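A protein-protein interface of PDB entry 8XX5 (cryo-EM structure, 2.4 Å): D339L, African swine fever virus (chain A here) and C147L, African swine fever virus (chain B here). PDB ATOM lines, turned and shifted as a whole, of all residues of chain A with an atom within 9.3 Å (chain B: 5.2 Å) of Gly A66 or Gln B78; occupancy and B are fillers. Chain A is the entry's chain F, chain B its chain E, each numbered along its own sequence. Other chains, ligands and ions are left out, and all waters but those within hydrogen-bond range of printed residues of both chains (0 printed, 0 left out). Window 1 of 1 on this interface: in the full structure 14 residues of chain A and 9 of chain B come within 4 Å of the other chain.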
ATOM      1  N   ILE A  13      10.044 -28.792  10.406  1.00  0.00           N
ATOM      2  CA  ILE A  13       9.807 -27.952  11.569  1.00  0.00           C
ATOM      3  C   ILE A  13       9.797 -26.503  11.107  1.00  0.00           C
ATOM      4  O   ILE A  13      10.843 -25.945  10.758  1.00  0.00           O
ATOM      5  CB  ILE A  13      10.865 -28.183  12.653  1.00  0.00           C
ATOM      6  CG1 ILE A  13      10.800 -29.624  13.157  1.00  0.00           C
ATOM      7  CG2 ILE A  13      10.650 -27.224  13.780  1.00  0.00           C
ATOM      8  CD1 ILE A  13      12.141 -30.214  13.472  1.00  0.00           C
ATOM      9  N   ASP A  14       8.614 -25.887  11.111  1.00  0.00           N
ATOM     10  CA  ASP A  14       8.484 -24.509  10.657  1.00  0.00           C
ATOM     11  C   ASP A  14       8.890 -23.493  11.715  1.00  0.00           C
ATOM     12  O   ASP A  14       9.137 -22.332  11.373  1.00  0.00           O
ATOM     13  CB  ASP A  14       7.050 -24.238  10.207  1.00  0.00           C
ATOM     14  CG  ASP A  14       6.704 -24.948   8.915  1.00  0.00           C
ATOM     15  OD1 ASP A  14       7.080 -26.130   8.766  1.00  0.00           O
ATOM     16  OD2 ASP A  14       6.058 -24.324   8.048  1.00  0.00           O
ATOM     17  N   ASP A  15       8.957 -23.892  12.982  1.00  0.00           N
ATOM     18  CA  ASP A  15       9.394 -23.011  14.066  1.00  0.00           C
ATOM     19  C   ASP A  15      10.374 -23.772  14.944  1.00  0.00           C
ATOM     20  O   ASP A  15      10.022 -24.249  16.029  1.00  0.00           O
ATOM     21  CB  ASP A  15       8.200 -22.502  14.877  1.00  0.00           C
ATOM     22  CG  ASP A  15       8.472 -21.165  15.534  1.00  0.00           C
ATOM     23  OD1 ASP A  15       9.563 -21.001  16.119  1.00  0.00           O
ATOM     24  OD2 ASP A  15       7.596 -20.278  15.468  1.00  0.00           O
ATOM     25  N   PRO A  16      11.624 -23.916  14.494  1.00  0.00           N
ATOM     26  CA  PRO A  16      12.584 -24.742  15.250  1.00  0.00           C
ATOM     27  C   PRO A  16      12.828 -24.270  16.671  1.00  0.00           C
ATOM     28  O   PRO A  16      13.009 -25.107  17.563  1.00  0.00           O
ATOM     29  CB  PRO A  16      13.860 -24.663  14.398  1.00  0.00           C
ATOM     30  CG  PRO A  16      13.676 -23.478  13.519  1.00  0.00           C
ATOM     31  CD  PRO A  16      12.213 -23.363  13.266  1.00  0.00           C
ATOM     32  N   THR A  17      12.845 -22.960  16.916  1.00  0.00           N
ATOM     33  CA  THR A  17      13.059 -22.477  18.276  1.00  0.00           C
ATOM     34  C   THR A  17      11.855 -22.768  19.165  1.00  0.00           C
ATOM     35  O   THR A  17      12.015 -23.111  20.341  1.00  0.00           O
ATOM     36  CB  THR A  17      13.383 -20.982  18.261  1.00  0.00           C
ATOM     37  OG1 THR A  17      13.253 -20.445  19.583  1.00  0.00           O
ATOM     38  CG2 THR A  17      12.463 -20.238  17.310  1.00  0.00           C
ATOM     39  N   ASN A  18      10.644 -22.638  18.623  1.00  0.00           N
ATOM     40  CA  ASN A  18       9.447 -22.986  19.379  1.00  0.00           C
ATOM     41  C   ASN A  18       9.237 -24.491  19.456  1.00  0.00           C
ATOM     42  O   ASN A  18       8.702 -24.984  20.453  1.00  0.00           O
ATOM     43  CB  ASN A  18       8.218 -22.321  18.761  1.00  0.00           C
ATOM     44  CG  ASN A  18       6.929 -23.008  19.153  1.00  0.00           C
ATOM     45  OD1 ASN A  18       6.549 -23.014  20.323  1.00  0.00           O
ATOM     46  ND2 ASN A  18       6.255 -23.603  18.178  1.00  0.00           N
ATOM     47  N   PHE A  19       9.630 -25.231  18.415  1.00  0.00           N
ATOM     48  CA  PHE A  19       9.526 -26.687  18.459  1.00  0.00           C
ATOM     49  C   PHE A  19      10.364 -27.267  19.585  1.00  0.00           C
ATOM     50  O   PHE A  19      10.030 -28.326  20.127  1.00  0.00           O
ATOM     51  CB  PHE A  19       9.954 -27.279  17.119  1.00  0.00           C
ATOM     52  CG  PHE A  19       9.948 -28.780  17.082  1.00  0.00           C
ATOM     53  CD1 PHE A  19       8.790 -29.471  16.779  1.00  0.00           C
ATOM     54  CD2 PHE A  19      11.105 -29.498  17.327  1.00  0.00           C
ATOM     55  CE1 PHE A  19       8.783 -30.847  16.735  1.00  0.00           C
ATOM     56  CE2 PHE A  19      11.103 -30.874  17.289  1.00  0.00           C
ATOM     57  CZ  PHE A  19       9.941 -31.550  16.991  1.00  0.00           C
ATOM     58  N   CYS A  20      11.445 -26.592  19.951  1.00  0.00           N
ATOM     59  CA  CYS A  20      12.198 -26.953  21.141  1.00  0.00           C
ATOM     60  C   CYS A  20      11.422 -26.467  22.365  1.00  0.00           C
ATOM     61  O   CYS A  20      10.247 -26.101  22.276  1.00  0.00           O
ATOM     62  CB  CYS A  20      13.612 -26.387  21.066  1.00  0.00           C
ATOM     63  SG  CYS A  20      14.575 -26.988  19.658  1.00  0.00           S
ATOM     64  N   CYS A  57      17.856 -31.159  15.613  1.00  0.00           N
ATOM     65  CA  CYS A  57      17.040 -30.318  14.738  1.00  0.00           C
ATOM     66  C   CYS A  57      17.968 -29.527  13.820  1.00  0.00           C
ATOM     67  O   CYS A  57      18.333 -28.378  14.082  1.00  0.00           O
ATOM     68  CB  CYS A  57      16.139 -29.402  15.555  1.00  0.00           C
ATOM     69  SG  CYS A  57      15.036 -28.369  14.565  1.00  0.00           S
ATOM     70  N   PHE A  58      18.362 -30.168  12.724  1.00  0.00           N
ATOM     71  CA  PHE A  58      19.188 -29.500  11.728  1.00  0.00           C
ATOM     72  C   PHE A  58      18.395 -28.395  11.046  1.00  0.00           C
ATOM     73  O   PHE A  58      17.210 -28.554  10.757  1.00  0.00           O
ATOM     74  CB  PHE A  58      19.673 -30.487  10.669  1.00  0.00           C
ATOM     75  CG  PHE A  58      20.315 -31.719  11.222  1.00  0.00           C
ATOM     76  CD1 PHE A  58      21.596 -31.679  11.731  1.00  0.00           C
ATOM     77  CD2 PHE A  58      19.647 -32.927  11.198  1.00  0.00           C
ATOM     78  CE1 PHE A  58      22.189 -32.816  12.231  1.00  0.00           C
ATOM     79  CE2 PHE A  58      20.237 -34.067  11.692  1.00  0.00           C
ATOM     80  CZ  PHE A  58      21.510 -34.012  12.210  1.00  0.00           C
ATOM     81  N   ILE A  59      19.059 -27.282  10.772  1.00  0.00           N
ATOM     82  CA  ILE A  59      18.444 -26.190  10.029  1.00  0.00           C
ATOM     83  C   ILE A  59      18.544 -26.488   8.541  1.00  0.00           C
ATOM     84  O   ILE A  59      19.569 -26.987   8.063  1.00  0.00           O
ATOM     85  CB  ILE A  59      19.113 -24.851  10.386  1.00  0.00           C
ATOM     86  CG1 ILE A  59      18.946 -24.560  11.876  1.00  0.00           C
ATOM     87  CG2 ILE A  59      18.524 -23.715   9.565  1.00  0.00           C
ATOM     88  CD1 ILE A  59      17.535 -24.755  12.370  1.00  0.00           C
ATOM     89  N   MET A  60      17.471 -26.202   7.804  1.00  0.00           N
ATOM     90  CA  MET A  60      17.475 -26.437   6.366  1.00  0.00           C
ATOM     91  C   MET A  60      18.585 -25.638   5.699  1.00  0.00           C
ATOM     92  O   MET A  60      18.755 -24.444   5.957  1.00  0.00           O
ATOM     93  CB  MET A  60      16.125 -26.070   5.753  1.00  0.00           C
ATOM     94  CG  MET A  60      15.125 -27.204   5.742  1.00  0.00           C
ATOM     95  SD  MET A  60      13.420 -26.642   5.783  1.00  0.00           S
ATOM     96  CE  MET A  60      12.624 -28.048   6.550  1.00  0.00           C
ATOM     97  N   ARG A  61      19.337 -26.308   4.832  1.00  0.00           N
ATOM     98  CA  ARG A  61      20.528 -25.737   4.224  1.00  0.00           C
ATOM     99  C   ARG A  61      20.296 -25.200   2.819  1.00  0.00           C
ATOM    100  O   ARG A  61      20.959 -24.239   2.422  1.00  0.00           O
ATOM    101  CB  ARG A  61      21.642 -26.789   4.185  1.00  0.00           C
ATOM    102  CG  ARG A  61      23.026 -26.235   3.948  1.00  0.00           C
ATOM    103  CD  ARG A  61      24.061 -27.345   3.912  1.00  0.00           C
ATOM    104  NE  ARG A  61      23.864 -28.260   2.793  1.00  0.00           N
ATOM    105  CZ  ARG A  61      24.029 -27.944   1.515  1.00  0.00           C
ATOM    106  NH1 ARG A  61      24.410 -26.733   1.144  1.00  0.00           N
ATOM    107  NH2 ARG A  61      23.809 -28.869   0.586  1.00  0.00           N
ATOM    108  N   THR A  62      19.369 -25.781   2.066  1.00  0.00           N
ATOM    109  CA  THR A  62      19.202 -25.454   0.657  1.00  0.00           C
ATOM    110  C   THR A  62      18.172 -24.361   0.407  1.00  0.00           C
ATOM    111  O   THR A  62      17.889 -24.054  -0.754  1.00  0.00           O
ATOM    112  CB  THR A  62      18.815 -26.708  -0.130  1.00  0.00           C
ATOM    113  OG1 THR A  62      17.701 -27.345   0.503  1.00  0.00           O
ATOM    114  CG2 THR A  62      19.981 -27.679  -0.175  1.00  0.00           C
ATOM    115  N   ASN A  63      17.608 -23.767   1.456  1.00  0.00           N
ATOM    116  CA  ASN A  63      16.688 -22.651   1.304  1.00  0.00           C
ATOM    117  C   ASN A  63      16.975 -21.626   2.391  1.00  0.00           C
ATOM    118  O   ASN A  63      17.713 -21.887   3.344  1.00  0.00           O
ATOM    119  CB  ASN A  63      15.223 -23.109   1.352  1.00  0.00           C
ATOM    120  CG  ASN A  63      14.938 -24.036   2.513  1.00  0.00           C
ATOM    121  OD1 ASN A  63      14.557 -23.593   3.594  1.00  0.00           O
ATOM    122  ND2 ASN A  63      15.118 -25.332   2.295  1.00  0.00           N
ATOM    123  N   ASN A  64      16.383 -20.442   2.235  1.00  0.00           N
ATOM    124  CA  ASN A  64      16.565 -19.337   3.165  1.00  0.00           C
ATOM    125  C   ASN A  64      15.376 -19.168   4.105  1.00  0.00           C
ATOM    126  O   ASN A  64      15.055 -18.044   4.506  1.00  0.00           O
ATOM    127  CB  ASN A  64      16.819 -18.039   2.398  1.00  0.00           C
ATOM    128  CG  ASN A  64      18.232 -17.948   1.860  1.00  0.00           C
ATOM    129  OD1 ASN A  64      19.086 -18.772   2.181  1.00  0.00           O
ATOM    130  ND2 ASN A  64      18.482 -16.943   1.030  1.00  0.00           N
ATOM    131  N   SER A  65      14.713 -20.266   4.464  1.00  0.00           N
ATOM    132  CA  SER A  65      13.533 -20.200   5.314  1.00  0.00           C
ATOM    133  C   SER A  65      13.854 -20.259   6.799  1.00  0.00           C
ATOM    134  O   SER A  65      13.046 -19.795   7.610  1.00  0.00           O
ATOM    135  CB  SER A  65      12.567 -21.336   4.965  1.00  0.00           C
ATOM    136  OG  SER A  65      13.191 -22.598   5.118  1.00  0.00           O
ATOM    137  N   GLY A  66      15.004 -20.814   7.174  1.00  0.00           N
ATOM    138  CA  GLY A  66      15.347 -20.962   8.572  1.00  0.00           C
ATOM    139  C   GLY A  66      14.674 -22.118   9.272  1.00  0.00           C
ATOM    140  O   GLY A  66      14.806 -22.245  10.493  1.00  0.00           O
ATOM    141  N   ARG A  67      13.958 -22.963   8.539  1.00  0.00           N
ATOM    142  CA  ARG A  67      13.237 -24.075   9.132  1.00  0.00           C
ATOM    143  C   ARG A  67      14.176 -25.247   9.407  1.00  0.00           C
ATOM    144  O   ARG A  67      15.256 -25.365   8.824  1.00  0.00           O
ATOM    145  CB  ARG A  67      12.099 -24.519   8.216  1.00  0.00           C
ATOM    146  CG  ARG A  67      10.945 -23.543   8.142  1.00  0.00           C
ATOM    147  CD  ARG A  67      10.300 -23.555   6.770  1.00  0.00           C
ATOM    148  NE  ARG A  67       9.928 -24.901   6.352  1.00  0.00           N
ATOM    149  CZ  ARG A  67      10.205 -25.419   5.164  1.00  0.00           C
ATOM    150  NH1 ARG A  67      10.862 -24.730   4.245  1.00  0.00           N
ATOM    151  NH2 ARG A  67       9.816 -26.660   4.891  1.00  0.00           N
ATOM    152  N   GLY A  68      13.747 -26.116  10.317  1.00  0.00           N
ATOM    153  CA  GLY A  68      14.486 -27.324  10.620  1.00  0.00           C
ATOM    154  C   GLY A  68      13.743 -28.556  10.154  1.00  0.00           C
ATOM    155  O   GLY A  68      12.554 -28.462   9.838  1.00  0.00           O
ATOM    156  N   TYR A  69      14.406 -29.710  10.077  1.00  0.00           N
ATOM    157  CA  TYR A  69      13.707 -30.920   9.660  1.00  0.00           C
ATOM    158  C   TYR A  69      13.717 -32.013  10.721  1.00  0.00           C
ATOM    159  O   TYR A  69      12.640 -32.475  11.110  1.00  0.00           O
ATOM    160  CB  TYR A  69      14.256 -31.451   8.326  1.00  0.00           C
ATOM    161  CG  TYR A  69      15.757 -31.457   8.139  1.00  0.00           C
ATOM    162  CD1 TYR A  69      16.458 -30.284   7.895  1.00  0.00           C
ATOM    163  CD2 TYR A  69      16.466 -32.650   8.152  1.00  0.00           C
ATOM    164  CE1 TYR A  69      17.820 -30.297   7.701  1.00  0.00           C
ATOM    165  CE2 TYR A  69      17.826 -32.671   7.959  1.00  0.00           C
ATOM    166  CZ  TYR A  69      18.498 -31.495   7.731  1.00  0.00           C
ATOM    167  OH  TYR A  69      19.859 -31.517   7.541  1.00  0.00           O
ATOM    168  N   ALA B  73      22.667 -15.340  10.235  1.00  0.00           N
ATOM    169  CA  ALA B  73      21.604 -15.392   9.237  1.00  0.00           C
ATOM    170  C   ALA B  73      20.477 -16.316   9.675  1.00  0.00           C
ATOM    171  O   ALA B  73      19.296 -15.978   9.535  1.00  0.00           O
ATOM    172  CB  ALA B  73      22.169 -15.835   7.890  1.00  0.00           C
ATOM    173  N   VAL B  74      20.820 -17.486  10.219  1.00  0.00           N
ATOM    174  CA  VAL B  74      19.804 -18.428  10.678  1.00  0.00           C
ATOM    175  C   VAL B  74      19.016 -17.832  11.835  1.00  0.00           C
ATOM    176  O   VAL B  74      17.781 -17.904  11.870  1.00  0.00           O
ATOM    177  CB  VAL B  74      20.456 -19.768  11.064  1.00  0.00           C
ATOM    178  CG1 VAL B  74      19.499 -20.613  11.888  1.00  0.00           C
ATOM    179  CG2 VAL B  74      20.897 -20.518   9.821  1.00  0.00           C
ATOM    180  N   ARG B  75      19.716 -17.225  12.796  1.00  0.00           N
ATOM    181  CA  ARG B  75      19.040 -16.633  13.943  1.00  0.00           C
ATOM    182  C   ARG B  75      18.124 -15.492  13.521  1.00  0.00           C
ATOM    183  O   ARG B  75      17.004 -15.371  14.026  1.00  0.00           O
ATOM    184  CB  ARG B  75      20.072 -16.149  14.961  1.00  0.00           C
ATOM    185  CG  ARG B  75      19.478 -15.686  16.274  1.00  0.00           C
ATOM    186  CD  ARG B  75      18.631 -16.769  16.912  1.00  0.00           C
ATOM    187  NE  ARG B  75      17.808 -16.239  17.992  1.00  0.00           N
ATOM    188  CZ  ARG B  75      16.562 -16.616  18.241  1.00  0.00           C
ATOM    189  NH1 ARG B  75      15.962 -17.541  17.510  1.00  0.00           N
ATOM    190  NH2 ARG B  75      15.904 -16.054  19.250  1.00  0.00           N
ATOM    191  N   ALA B  76      18.577 -14.650  12.592  1.00  0.00           N
ATOM    192  CA  ALA B  76      17.755 -13.531  12.146  1.00  0.00           C
ATOM    193  C   ALA B  76      16.547 -14.009  11.350  1.00  0.00           C
ATOM    194  O   ALA B  76      15.446 -13.466  11.494  1.00  0.00           O
ATOM    195  CB  ALA B  76      18.602 -12.559  11.328  1.00  0.00           C
ATOM    196  N   GLN B  77      16.723 -15.035  10.515  1.00  0.00           N
ATOM    197  CA  GLN B  77      15.582 -15.586   9.795  1.00  0.00           C
ATOM    198  C   GLN B  77      14.577 -16.211  10.753  1.00  0.00           C
ATOM    199  O   GLN B  77      13.364 -16.119  10.535  1.00  0.00           O
ATOM    200  CB  GLN B  77      16.054 -16.610   8.766  1.00  0.00           C
ATOM    201  CG  GLN B  77      14.952 -17.137   7.865  1.00  0.00           C
ATOM    202  CD  GLN B  77      14.113 -16.033   7.259  1.00  0.00           C
ATOM    203  OE1 GLN B  77      14.640 -15.049   6.742  1.00  0.00           O
ATOM    204  NE2 GLN B  77      12.798 -16.189   7.321  1.00  0.00           N
ATOM    205  N   GLN B  78      15.060 -16.859  11.813  1.00  0.00           N
ATOM    206  CA  GLN B  78      14.151 -17.431  12.797  1.00  0.00           C
ATOM    207  C   GLN B  78      13.433 -16.343  13.586  1.00  0.00           C
ATOM    208  O   GLN B  78      12.248 -16.480  13.905  1.00  0.00           O
ATOM    209  CB  GLN B  78      14.915 -18.369  13.726  1.00  0.00           C
ATOM    210  CG  GLN B  78      15.199 -19.721  13.107  1.00  0.00           C
ATOM    211  CD  GLN B  78      16.217 -20.515  13.887  1.00  0.00           C
ATOM    212  OE1 GLN B  78      16.743 -20.048  14.895  1.00  0.00           O
ATOM    213  NE2 GLN B  78      16.503 -21.723  13.425  1.00  0.00           N
ATOM    214  N   LEU B  79      14.134 -15.252  13.906  1.00  0.00           N
ATOM    215  CA  LEU B  79      13.497 -14.109  14.548  1.00  0.00           C
ATOM    216  C   LEU B  79      12.533 -13.391  13.618  1.00  0.00           C
ATOM    217  O   LEU B  79      11.712 -12.601  14.089  1.00  0.00           O
ATOM    218  CB  LEU B  79      14.551 -13.122  15.048  1.00  0.00           C
ATOM    219  CG  LEU B  79      15.426 -13.573  16.216  1.00  0.00           C
ATOM    220  CD1 LEU B  79      16.789 -12.910  16.136  1.00  0.00           C
ATOM    221  CD2 LEU B  79      14.748 -13.258  17.537  1.00  0.00           C
ATOM    222  N   ALA B  80      12.648 -13.607  12.309  1.00  0.00           N
ATOM    223  CA  ALA B  80      11.655 -13.056  11.394  1.00  0.00           C
ATOM    224  C   ALA B  80      10.281 -13.678  11.628  1.00  0.00           C
ATOM    225  O   ALA B  80       9.274 -12.965  11.679  1.00  0.00           O
ATOM    226  CB  ALA B  80      12.099 -13.259   9.947  1.00  0.00           C
ATOM    227  N   ILE B  81      10.218 -14.995  11.802  1.00  0.00           N
ATOM    228  CA  ILE B  81       8.934 -15.655  12.023  1.00  0.00           C
ATOM    229  C   ILE B  81       8.591 -15.724  13.510  1.00  0.00           C
ATOM    230  O   ILE B  81       7.446 -15.494  13.900  1.00  0.00           O
ATOM    231  CB  ILE B  81       8.936 -17.053  11.364  1.00  0.00           C
ATOM    232  CG1 ILE B  81       9.997 -17.965  11.985  1.00  0.00           C
ATOM    233  CG2 ILE B  81       9.162 -16.933   9.864  1.00  0.00           C
ATOM    234  CD1 ILE B  81       9.420 -19.096  12.805  1.00  0.00           C
ATOM    235  N   ASN B  82       9.576 -16.042  14.343  1.00  0.00           N
ATOM    236  CA  ASN B  82       9.510 -15.926  15.795  1.00  0.00           C
ATOM    237  C   ASN B  82       9.918 -14.516  16.195  1.00  0.00           C
ATOM    238  O   ASN B  82       9.693 -13.568  15.440  1.00  0.00           O
ATOM    239  CB  ASN B  82      10.377 -16.975  16.488  1.00  0.00           C
ATOM    240  CG  ASN B  82       9.762 -17.463  17.785  1.00  0.00           C
ATOM    241  OD1 ASN B  82       9.398 -16.666  18.648  1.00  0.00           O
ATOM    242  ND2 ASN B  82       9.624 -18.775  17.921  1.00  0.00           N
ATOM    243  N   GLY B  83      10.465 -14.355  17.394  1.00  0.00           N
ATOM    244  CA  GLY B  83      10.751 -13.034  17.913  1.00  0.00           C
ATOM    245  C   GLY B  83      10.776 -12.983  19.423  1.00  0.00           C
ATOM    246  O   GLY B  83      11.106 -11.948  20.010  1.00  0.00           O
ATOM    247  N   LEU B 109      21.682 -21.540  18.948  1.00  0.00           N
ATOM    248  CA  LEU B 109      22.094 -22.485  17.924  1.00  0.00           C
ATOM    249  C   LEU B 109      23.405 -23.163  18.304  1.00  0.00           C
ATOM    250  O   LEU B 109      24.143 -22.702  19.176  1.00  0.00           O
ATOM    251  CB  LEU B 109      22.241 -21.784  16.573  1.00  0.00           C
ATOM    252  CG  LEU B 109      21.057 -20.929  16.123  1.00  0.00           C
ATOM    253  CD1 LEU B 109      21.509 -19.857  15.151  1.00  0.00           C
ATOM    254  CD2 LEU B 109      19.984 -21.801  15.501  1.00  0.00           C
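Ile B81 touches Asp A14 (CD1 to O, 3.5 Å). CD1 of Ile B81 touches OD2 of Asp A15, 3.4 Å away. Gln B78 touches Pro A16. Asn B82 touches Thr A17. CB of Asn A18 touches ND2 of Asn B82, 3.9 Å away. CG1 of Ile A59 touches CG1 of Val B74 (3.99 Å). Ile A59 touches Gln B78. Asn A64 touches Gln B77 (O to CG, 3.5 Å). CG of Gln B77 touches O of Ser A65 (3.3 Å). Gly A66 touches Gln B77.
The backbone carbonyl oxygen (O) of Pro A16 sits at hydrogen-bond distance from the side-chain sulfur (SG) of Cys A20 (3.2 Å). The side-chain amide oxygen of Asn A63 lies close to the backbone NH of Ser A65 (3.4 Å). NE of Arg A67 is in salt-bridge range of OD1 of Asp A14 (3.9 Å). NH1 of Arg A67 is in hydrogen-bond range of OG of Ser A65. N of Asn A18 sits at hydrogen-bond distance from OD1 of Asp A15, at 3.2 Å.
Printed residues of chain B that touch a printed residue of chain A: Val B74, Gln B77, Gln B78, Ile B81 and Asn B82. Among the printed residues, 12 pairs touch across the chains.
The side-chain amide nitrogen (NE2) of Gln B78 is in hydrogen-bond range of the backbone carbonyl oxygen (O) of Gly A66, 3.4 Å away. OD1 of Asp A15 sits at hydrogen-bond distance from ND2 of Asn B82 (2.9 Å).
Of chain B, only Gln B77 and Gln B78 come within 4 Å of Gly A66. No residue of chain A comes within 4 Å of Ala B80. Of the printed residues of chain B, Ser A65 touches Gln B77 (3.3 Å). Of the printed residues of chain B, Asn A18 touches Asn B82. Of the printed residues of chain B, Pro A16 touches Gln B78 (3.3 Å). Of the printed residues of chain A, Gln B77 touches Asn A64, Ser A65 and Gly A66. Of the printed residues of chain B, Thr A17 touches Asn B82. The nearest residue of chain B that does not touch Gly A66 is Val B74 (5.1 Å).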
